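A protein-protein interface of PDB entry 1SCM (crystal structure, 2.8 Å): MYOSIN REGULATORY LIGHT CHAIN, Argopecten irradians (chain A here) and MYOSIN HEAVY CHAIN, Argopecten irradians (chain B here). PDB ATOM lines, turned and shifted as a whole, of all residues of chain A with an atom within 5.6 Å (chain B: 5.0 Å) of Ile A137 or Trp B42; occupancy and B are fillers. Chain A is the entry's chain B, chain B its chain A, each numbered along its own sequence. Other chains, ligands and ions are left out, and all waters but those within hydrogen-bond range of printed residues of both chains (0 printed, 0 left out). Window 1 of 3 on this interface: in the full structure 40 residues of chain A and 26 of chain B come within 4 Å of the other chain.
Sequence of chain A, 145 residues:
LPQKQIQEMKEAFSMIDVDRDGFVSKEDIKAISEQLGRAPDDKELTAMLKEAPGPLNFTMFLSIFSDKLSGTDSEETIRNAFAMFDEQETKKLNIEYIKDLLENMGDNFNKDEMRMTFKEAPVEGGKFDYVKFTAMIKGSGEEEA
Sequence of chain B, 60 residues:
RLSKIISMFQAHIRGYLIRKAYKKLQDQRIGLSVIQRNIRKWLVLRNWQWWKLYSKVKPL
The side-chain carboxylate (OE1) of Glu A120 is in salt-bridge range of the guanidinium group (NH2) of Arg B46 (3.5 Å).
The backbone carbonyl oxygen (O) of Ile A78 lies within hydrogen-bond range of the side-chain hydroxyl (OG1) of Thr A134.
Ile A78 touches Asn B38 (CD1 to ND2, 3.3 Å).
CD1 of Leu B43 touches CB of Met A116, at 3.6 Å.
CG2 of Ile B39 touches OG1 of Thr A117 (3.5 Å).
OG1 of Thr A117 touches CD2 of Leu B43 (3.6 Å).
CE2 of Phe A133 touches CD1 of Ile B39, at 3.5 Å.
Phe A133 touches Trp B42 (CE1 to CZ3, 3.998 Å).
Trp B42 touches Met A136.
Asn B38 touches Ile A137 (O to CD1, 3.5 Å).
Ile B39 touches Ile A137 (CG1 to CD1, 3.4 Å).
O of Ile A137 touches CD1 of Trp B42, at 3.1 Å.
Of chain B, only Asn B38 (3.5 Å), Ile B39 (3.4 Å) and Trp B42 (3.1 Å) come within 4 Å of Ile A137.
Of the printed residues of chain A, Trp B42 touches Phe A133 (3.998 Å), Met A136 (3.7 Å) and Ile A137 (3.1 Å).
Of the printed residues of chain B, Thr A117 touches Ile B39 and Leu B43.
Printed residues of chain A within 4 Å of Asn B38: Ile A78 (3.3 Å) and Ile A137 (3.5 Å).
Of the printed residues of chain B, Glu A120 touches Arg B46.
Of the printed residues of chain A, Leu B43 touches Met A116 and Thr A117.
Of the printed residues of chain B, Ile A78 touches Asn B38 (3.3 Å).
Thr A134 touches none of the printed residues of chain B.
The nearest residue of chain B that does not touch Ile A137 is Ile B35 (4.8 Å).
The nearest printed residue of chain A that does not touch Trp B42 is Thr A117 (4.4 Å).
The nearest printed residue of chain B that does not touch Glu A120 is Trp B42 (5.2 Å).
Of the 11 printed residues of chain A, 7 touch a printed residue of chain B.
Hydrophobic or aromatic side chains of chain A within 4 Å of the printed part of chain B: Ile A78, Met A116, Phe A133 and Ile A137.
Along chain A the printed residues that touch a printed residue of chain B span positions 78 to 137.
Of the 10 printed residues of chain B, 5 touch a printed residue of chain A.
Printed residues of chain B that touch a printed residue of chain A: Asn B38, Ile B39, Trp B42, Leu B43 and Arg B46.
Along chain B the printed residues that touch a printed residue of chain A span positions 38 to 46.
Among the printed residues, Asp or Glu carboxylates within 4 Å of a Lys or Arg side-chain nitrogen of the other chain: Glu A120 with Arg B46 (3.5 Å).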
ATOM      1  N   ILE A  78      11.174   5.959 -13.020  1.00  0.00           N
ATOM      2  CA  ILE A  78      12.442   6.027 -12.284  1.00  0.00           C
ATOM      3  C   ILE A  78      13.580   6.439 -13.218  1.00  0.00           C
ATOM      4  O   ILE A  78      14.667   5.868 -13.163  1.00  0.00           O
ATOM      5  CB  ILE A  78      12.826   4.668 -11.657  1.00  0.00           C
ATOM      6  CG1 ILE A  78      11.680   3.862 -11.142  1.00  0.00           C
ATOM      7  CG2 ILE A  78      13.738   4.999 -10.480  1.00  0.00           C
ATOM      8  CD1 ILE A  78      12.163   2.633 -10.335  1.00  0.00           C
ATOM      9  N   MET A 116      24.955   0.212   0.447  1.00  0.00           N
ATOM     10  CA  MET A 116      24.323  -0.860  -0.303  1.00  0.00           C
ATOM     11  C   MET A 116      23.932  -0.401  -1.672  1.00  0.00           C
ATOM     12  O   MET A 116      24.073  -1.145  -2.643  1.00  0.00           O
ATOM     13  CB  MET A 116      23.050  -1.389   0.358  1.00  0.00           C
ATOM     14  CG  MET A 116      23.189  -2.107   1.711  1.00  0.00           C
ATOM     15  SD  MET A 116      24.539  -3.312   1.861  1.00  0.00           S
ATOM     16  CE  MET A 116      24.221  -4.465   0.545  1.00  0.00           C
ATOM     17  N   THR A 117      23.519   0.865  -1.731  1.00  0.00           N
ATOM     18  CA  THR A 117      23.066   1.445  -2.966  1.00  0.00           C
ATOM     19  C   THR A 117      24.223   1.516  -3.930  1.00  0.00           C
ATOM     20  O   THR A 117      24.006   1.342  -5.118  1.00  0.00           O
ATOM     21  CB  THR A 117      22.534   2.818  -2.643  1.00  0.00           C
ATOM     22  OG1 THR A 117      21.331   2.574  -1.915  1.00  0.00           O
ATOM     23  CG2 THR A 117      22.317   3.682  -3.859  1.00  0.00           C
ATOM     24  N   GLU A 120      26.924  -2.248  -6.054  1.00  0.00           N
ATOM     25  CA  GLU A 120      26.826  -2.685  -7.448  1.00  0.00           C
ATOM     26  C   GLU A 120      26.492  -1.585  -8.469  1.00  0.00           C
ATOM     27  O   GLU A 120      26.215  -1.914  -9.622  1.00  0.00           O
ATOM     28  CB  GLU A 120      25.748  -3.781  -7.580  1.00  0.00           C
ATOM     29  CG  GLU A 120      26.131  -5.263  -7.441  1.00  0.00           C
ATOM     30  CD  GLU A 120      26.158  -5.867  -6.039  1.00  0.00           C
ATOM     31  OE1 GLU A 120      25.471  -5.350  -5.146  1.00  0.00           O
ATOM     32  OE2 GLU A 120      26.854  -6.875  -5.855  1.00  0.00           O
ATOM     33  N   LYS A 132      21.170   2.534 -16.686  1.00  0.00           N
ATOM     34  CA  LYS A 132      21.579   1.210 -16.276  1.00  0.00           C
ATOM     35  C   LYS A 132      21.184   1.004 -14.849  1.00  0.00           C
ATOM     36  O   LYS A 132      20.348   0.139 -14.658  1.00  0.00           O
ATOM     37  CB  LYS A 132      23.053   1.042 -16.371  1.00  0.00           C
ATOM     38  CG  LYS A 132      23.344  -0.267 -16.995  1.00  0.00           C
ATOM     39  CD  LYS A 132      24.180  -0.971 -15.979  1.00  0.00           C
ATOM     40  CE  LYS A 132      23.717  -2.415 -15.919  1.00  0.00           C
ATOM     41  NZ  LYS A 132      22.327  -2.538 -15.500  1.00  0.00           N
ATOM     42  N   PHE A 133      21.712   1.709 -13.830  1.00  0.00           N
ATOM     43  CA  PHE A 133      21.248   1.545 -12.447  1.00  0.00           C
ATOM     44  C   PHE A 133      19.744   1.386 -12.337  1.00  0.00           C
ATOM     45  O   PHE A 133      19.332   0.463 -11.667  1.00  0.00           O
ATOM     46  CB  PHE A 133      21.611   2.736 -11.560  1.00  0.00           C
ATOM     47  CG  PHE A 133      21.131   2.557 -10.120  1.00  0.00           C
ATOM     48  CD1 PHE A 133      21.732   1.611  -9.296  1.00  0.00           C
ATOM     49  CD2 PHE A 133      20.071   3.307  -9.636  1.00  0.00           C
ATOM     50  CE1 PHE A 133      21.275   1.418  -8.002  1.00  0.00           C
ATOM     51  CE2 PHE A 133      19.614   3.113  -8.341  1.00  0.00           C
ATOM     52  CZ  PHE A 133      20.210   2.169  -7.525  1.00  0.00           C
ATOM     53  N   THR A 134      18.930   2.251 -12.955  1.00  0.00           N
ATOM     54  CA  THR A 134      17.500   2.063 -12.998  1.00  0.00           C
ATOM     55  C   THR A 134      17.192   0.708 -13.585  1.00  0.00           C
ATOM     56  O   THR A 134      16.519   0.009 -12.839  1.00  0.00           O
ATOM     57  CB  THR A 134      16.742   3.033 -13.868  1.00  0.00           C
ATOM     58  OG1 THR A 134      17.067   4.345 -13.468  1.00  0.00           O
ATOM     59  CG2 THR A 134      15.245   2.823 -13.704  1.00  0.00           C
ATOM     60  N   ALA A 135      17.590   0.255 -14.797  1.00  0.00           N
ATOM     61  CA  ALA A 135      17.291  -1.131 -15.227  1.00  0.00           C
ATOM     62  C   ALA A 135      17.519  -2.199 -14.128  1.00  0.00           C
ATOM     63  O   ALA A 135      16.625  -2.965 -13.744  1.00  0.00           O
ATOM     64  CB  ALA A 135      18.159  -1.531 -16.405  1.00  0.00           C
ATOM     65  N   MET A 136      18.700  -2.126 -13.510  1.00  0.00           N
ATOM     66  CA  MET A 136      19.072  -2.963 -12.393  1.00  0.00           C
ATOM     67  C   MET A 136      18.123  -2.836 -11.210  1.00  0.00           C
ATOM     68  O   MET A 136      17.619  -3.868 -10.803  1.00  0.00           O
ATOM     69  CB  MET A 136      20.474  -2.581 -11.994  1.00  0.00           C
ATOM     70  CG  MET A 136      21.046  -3.190 -10.707  1.00  0.00           C
ATOM     71  SD  MET A 136      22.575  -2.348 -10.244  1.00  0.00           S
ATOM     72  CE  MET A 136      23.481  -2.421 -11.762  1.00  0.00           C
ATOM     73  N   ILE A 137      17.899  -1.657 -10.610  1.00  0.00           N
ATOM     74  CA  ILE A 137      16.981  -1.422  -9.503  1.00  0.00           C
ATOM     75  C   ILE A 137      15.616  -2.030  -9.753  1.00  0.00           C
ATOM     76  O   ILE A 137      14.962  -2.553  -8.862  1.00  0.00           O
ATOM     77  CB  ILE A 137      16.852   0.127  -9.260  1.00  0.00           C
ATOM     78  CG1 ILE A 137      16.141   0.389  -8.005  1.00  0.00           C
ATOM     79  CG2 ILE A 137      15.865   0.826 -10.155  1.00  0.00           C
ATOM     80  CD1 ILE A 137      16.150   1.904  -7.711  1.00  0.00           C
ATOM     81  N   LYS A 138      15.271  -2.041 -11.030  1.00  0.00           N
ATOM     82  CA  LYS A 138      13.942  -2.313 -11.465  1.00  0.00           C
ATOM     83  C   LYS A 138      13.639  -3.743 -11.831  1.00  0.00           C
ATOM     84  O   LYS A 138      14.032  -4.699 -11.165  1.00  0.00           O
ATOM     85  CB  LYS A 138      13.743  -1.296 -12.607  1.00  0.00           C
ATOM     86  CG  LYS A 138      12.557  -0.359 -12.452  1.00  0.00           C
ATOM     87  CD  LYS A 138      11.167  -0.813 -12.921  1.00  0.00           C
ATOM     88  CE  LYS A 138      10.385  -1.770 -12.008  1.00  0.00           C
ATOM     89  NZ  LYS A 138       9.993  -1.145 -10.765  1.00  0.00           N
ATOM     90  N   ILE B  35      13.060   8.521  -6.849  1.00  0.00           N
ATOM     91  CA  ILE B  35      14.393   7.905  -6.781  1.00  0.00           C
ATOM     92  C   ILE B  35      14.612   7.159  -5.458  1.00  0.00           C
ATOM     93  O   ILE B  35      14.855   5.953  -5.506  1.00  0.00           O
ATOM     94  CB  ILE B  35      15.530   8.994  -6.976  1.00  0.00           C
ATOM     95  CG1 ILE B  35      15.512   9.629  -8.367  1.00  0.00           C
ATOM     96  CG2 ILE B  35      16.880   8.320  -6.831  1.00  0.00           C
ATOM     97  CD1 ILE B  35      16.610  10.676  -8.551  1.00  0.00           C
ATOM     98  N   ASN B  38      11.901   3.996  -4.677  1.00  0.00           N
ATOM     99  CA  ASN B  38      12.276   2.809  -5.413  1.00  0.00           C
ATOM    100  C   ASN B  38      13.661   2.298  -5.107  1.00  0.00           C
ATOM    101  O   ASN B  38      13.790   1.088  -5.214  1.00  0.00           O
ATOM    102  CB  ASN B  38      12.128   3.060  -6.891  1.00  0.00           C
ATOM    103  CG  ASN B  38      10.649   3.245  -7.220  1.00  0.00           C
ATOM    104  OD1 ASN B  38       9.760   2.609  -6.654  1.00  0.00           O
ATOM    105  ND2 ASN B  38      10.278   4.125  -8.134  1.00  0.00           N
ATOM    106  N   ILE B  39      14.714   3.026  -4.704  1.00  0.00           N
ATOM    107  CA  ILE B  39      15.936   2.337  -4.253  1.00  0.00           C
ATOM    108  C   ILE B  39      15.692   1.634  -2.919  1.00  0.00           C
ATOM    109  O   ILE B  39      16.289   0.593  -2.619  1.00  0.00           O
ATOM    110  CB  ILE B  39      17.105   3.296  -4.065  1.00  0.00           C
ATOM    111  CG1 ILE B  39      17.405   4.031  -5.374  1.00  0.00           C
ATOM    112  CG2 ILE B  39      18.318   2.477  -3.632  1.00  0.00           C
ATOM    113  CD1 ILE B  39      18.635   4.933  -5.460  1.00  0.00           C
ATOM    114  N   ARG B  40      14.769   2.173  -2.124  1.00  0.00           N
ATOM    115  CA  ARG B  40      14.420   1.586  -0.854  1.00  0.00           C
ATOM    116  C   ARG B  40      13.633   0.289  -1.024  1.00  0.00           C
ATOM    117  O   ARG B  40      13.742  -0.634  -0.216  1.00  0.00           O
ATOM    118  CB  ARG B  40      13.655   2.651  -0.090  1.00  0.00           C
ATOM    119  CG  ARG B  40      14.695   3.431   0.695  1.00  0.00           C
ATOM    120  CD  ARG B  40      14.157   4.531   1.620  1.00  0.00           C
ATOM    121  NE  ARG B  40      14.907   4.649   2.859  1.00  0.00           N
ATOM    122  CZ  ARG B  40      15.328   5.835   3.332  1.00  0.00           C
ATOM    123  NH1 ARG B  40      15.107   6.957   2.664  1.00  0.00           N
ATOM    124  NH2 ARG B  40      15.816   5.929   4.579  1.00  0.00           N
ATOM    125  N   LYS B  41      12.863   0.235  -2.131  1.00  0.00           N
ATOM    126  CA  LYS B  41      12.042  -0.910  -2.545  1.00  0.00           C
ATOM    127  C   LYS B  41      12.866  -2.115  -2.964  1.00  0.00           C
ATOM    128  O   LYS B  41      12.529  -3.265  -2.677  1.00  0.00           O
ATOM    129  CB  LYS B  41      11.154  -0.527  -3.717  1.00  0.00           C
ATOM    130  CG  LYS B  41       9.795  -1.158  -3.526  1.00  0.00           C
ATOM    131  CD  LYS B  41       9.039  -0.508  -2.359  1.00  0.00           C
ATOM    132  CE  LYS B  41       7.796  -1.323  -1.953  1.00  0.00           C
ATOM    133  NZ  LYS B  41       6.761  -1.371  -2.975  1.00  0.00           N
ATOM    134  N   TRP B  42      13.969  -1.795  -3.642  1.00  0.00           N
ATOM    135  CA  TRP B  42      14.967  -2.727  -4.145  1.00  0.00           C
ATOM    136  C   TRP B  42      15.849  -3.289  -3.048  1.00  0.00           C
ATOM    137  O   TRP B  42      15.969  -4.502  -2.936  1.00  0.00           O
ATOM    138  CB  TRP B  42      15.771  -1.976  -5.167  1.00  0.00           C
ATOM    139  CG  TRP B  42      16.927  -2.688  -5.830  1.00  0.00           C
ATOM    140  CD1 TRP B  42      16.726  -3.756  -6.669  1.00  0.00           C
ATOM    141  CD2 TRP B  42      18.244  -2.302  -5.710  1.00  0.00           C
ATOM    142  NE1 TRP B  42      17.933  -4.036  -7.107  1.00  0.00           N
ATOM    143  CE2 TRP B  42      18.868  -3.213  -6.569  1.00  0.00           C
ATOM    144  CE3 TRP B  42      18.997  -1.340  -5.025  1.00  0.00           C
ATOM    145  CZ2 TRP B  42      20.259  -3.154  -6.741  1.00  0.00           C
ATOM    146  CZ3 TRP B  42      20.376  -1.296  -5.207  1.00  0.00           C
ATOM    147  CH2 TRP B  42      21.007  -2.195  -6.058  1.00  0.00           C
ATOM    148  N   LEU B  43      16.486  -2.442  -2.239  1.00  0.00           N
ATOM    149  CA  LEU B  43      17.275  -2.892  -1.109  1.00  0.00           C
ATOM    150  C   LEU B  43      16.497  -3.923  -0.273  1.00  0.00           C
ATOM    151  O   LEU B  43      17.019  -4.976   0.088  1.00  0.00           O
ATOM    152  CB  LEU B  43      17.668  -1.566  -0.385  1.00  0.00           C
ATOM    153  CG  LEU B  43      19.151  -0.984  -0.256  1.00  0.00           C
ATOM    154  CD1 LEU B  43      20.004  -1.357  -1.470  1.00  0.00           C
ATOM    155  CD2 LEU B  43      19.085   0.545  -0.054  1.00  0.00           C
ATOM    156  N   VAL B  44      15.203  -3.693  -0.059  1.00  0.00           N
ATOM    157  CA  VAL B  44      14.302  -4.680   0.561  1.00  0.00           C
ATOM    158  C   VAL B  44      14.240  -6.032  -0.146  1.00  0.00           C
ATOM    159  O   VAL B  44      14.541  -7.039   0.474  1.00  0.00           O
ATOM    160  CB  VAL B  44      12.837  -4.104   0.662  1.00  0.00           C
ATOM    161  CG1 VAL B  44      11.866  -5.178   1.070  1.00  0.00           C
ATOM    162  CG2 VAL B  44      12.750  -3.049   1.766  1.00  0.00           C
ATOM    163  N   LEU B  45      13.856  -6.049  -1.420  1.00  0.00           N
ATOM    164  CA  LEU B  45      13.786  -7.235  -2.273  1.00  0.00           C
ATOM    165  C   LEU B  45      14.886  -8.257  -2.116  1.00  0.00           C
ATOM    166  O   LEU B  45      14.672  -9.438  -1.827  1.00  0.00           O
ATOM    167  CB  LEU B  45      13.797  -6.853  -3.768  1.00  0.00           C
ATOM    168  CG  LEU B  45      12.509  -6.873  -4.561  1.00  0.00           C
ATOM    169  CD1 LEU B  45      12.140  -8.330  -4.795  1.00  0.00           C
ATOM    170  CD2 LEU B  45      11.410  -6.061  -3.831  1.00  0.00           C
ATOM    171  N   ARG B  46      16.073  -7.702  -2.305  1.00  0.00           N
ATOM    172  CA  ARG B  46      17.312  -8.440  -2.328  1.00  0.00           C
ATOM    173  C   ARG B  46      17.675  -8.922  -0.974  1.00  0.00           C
ATOM    174  O   ARG B  46      18.636  -9.675  -0.900  1.00  0.00           O
ATOM    175  CB  ARG B  46      18.459  -7.617  -2.744  1.00  0.00           C
ATOM    176  CG  ARG B  46      18.220  -6.603  -3.817  1.00  0.00           C
ATOM    177  CD  ARG B  46      19.335  -5.640  -3.527  1.00  0.00           C
ATOM    178  NE  ARG B  46      20.604  -6.221  -3.920  1.00  0.00           N
ATOM    179  CZ  ARG B  46      21.616  -6.377  -3.072  1.00  0.00           C
ATOM    180  NH1 ARG B  46      21.530  -6.013  -1.786  1.00  0.00           N
ATOM    181  NH2 ARG B  46      22.724  -6.931  -3.559  1.00  0.00           N
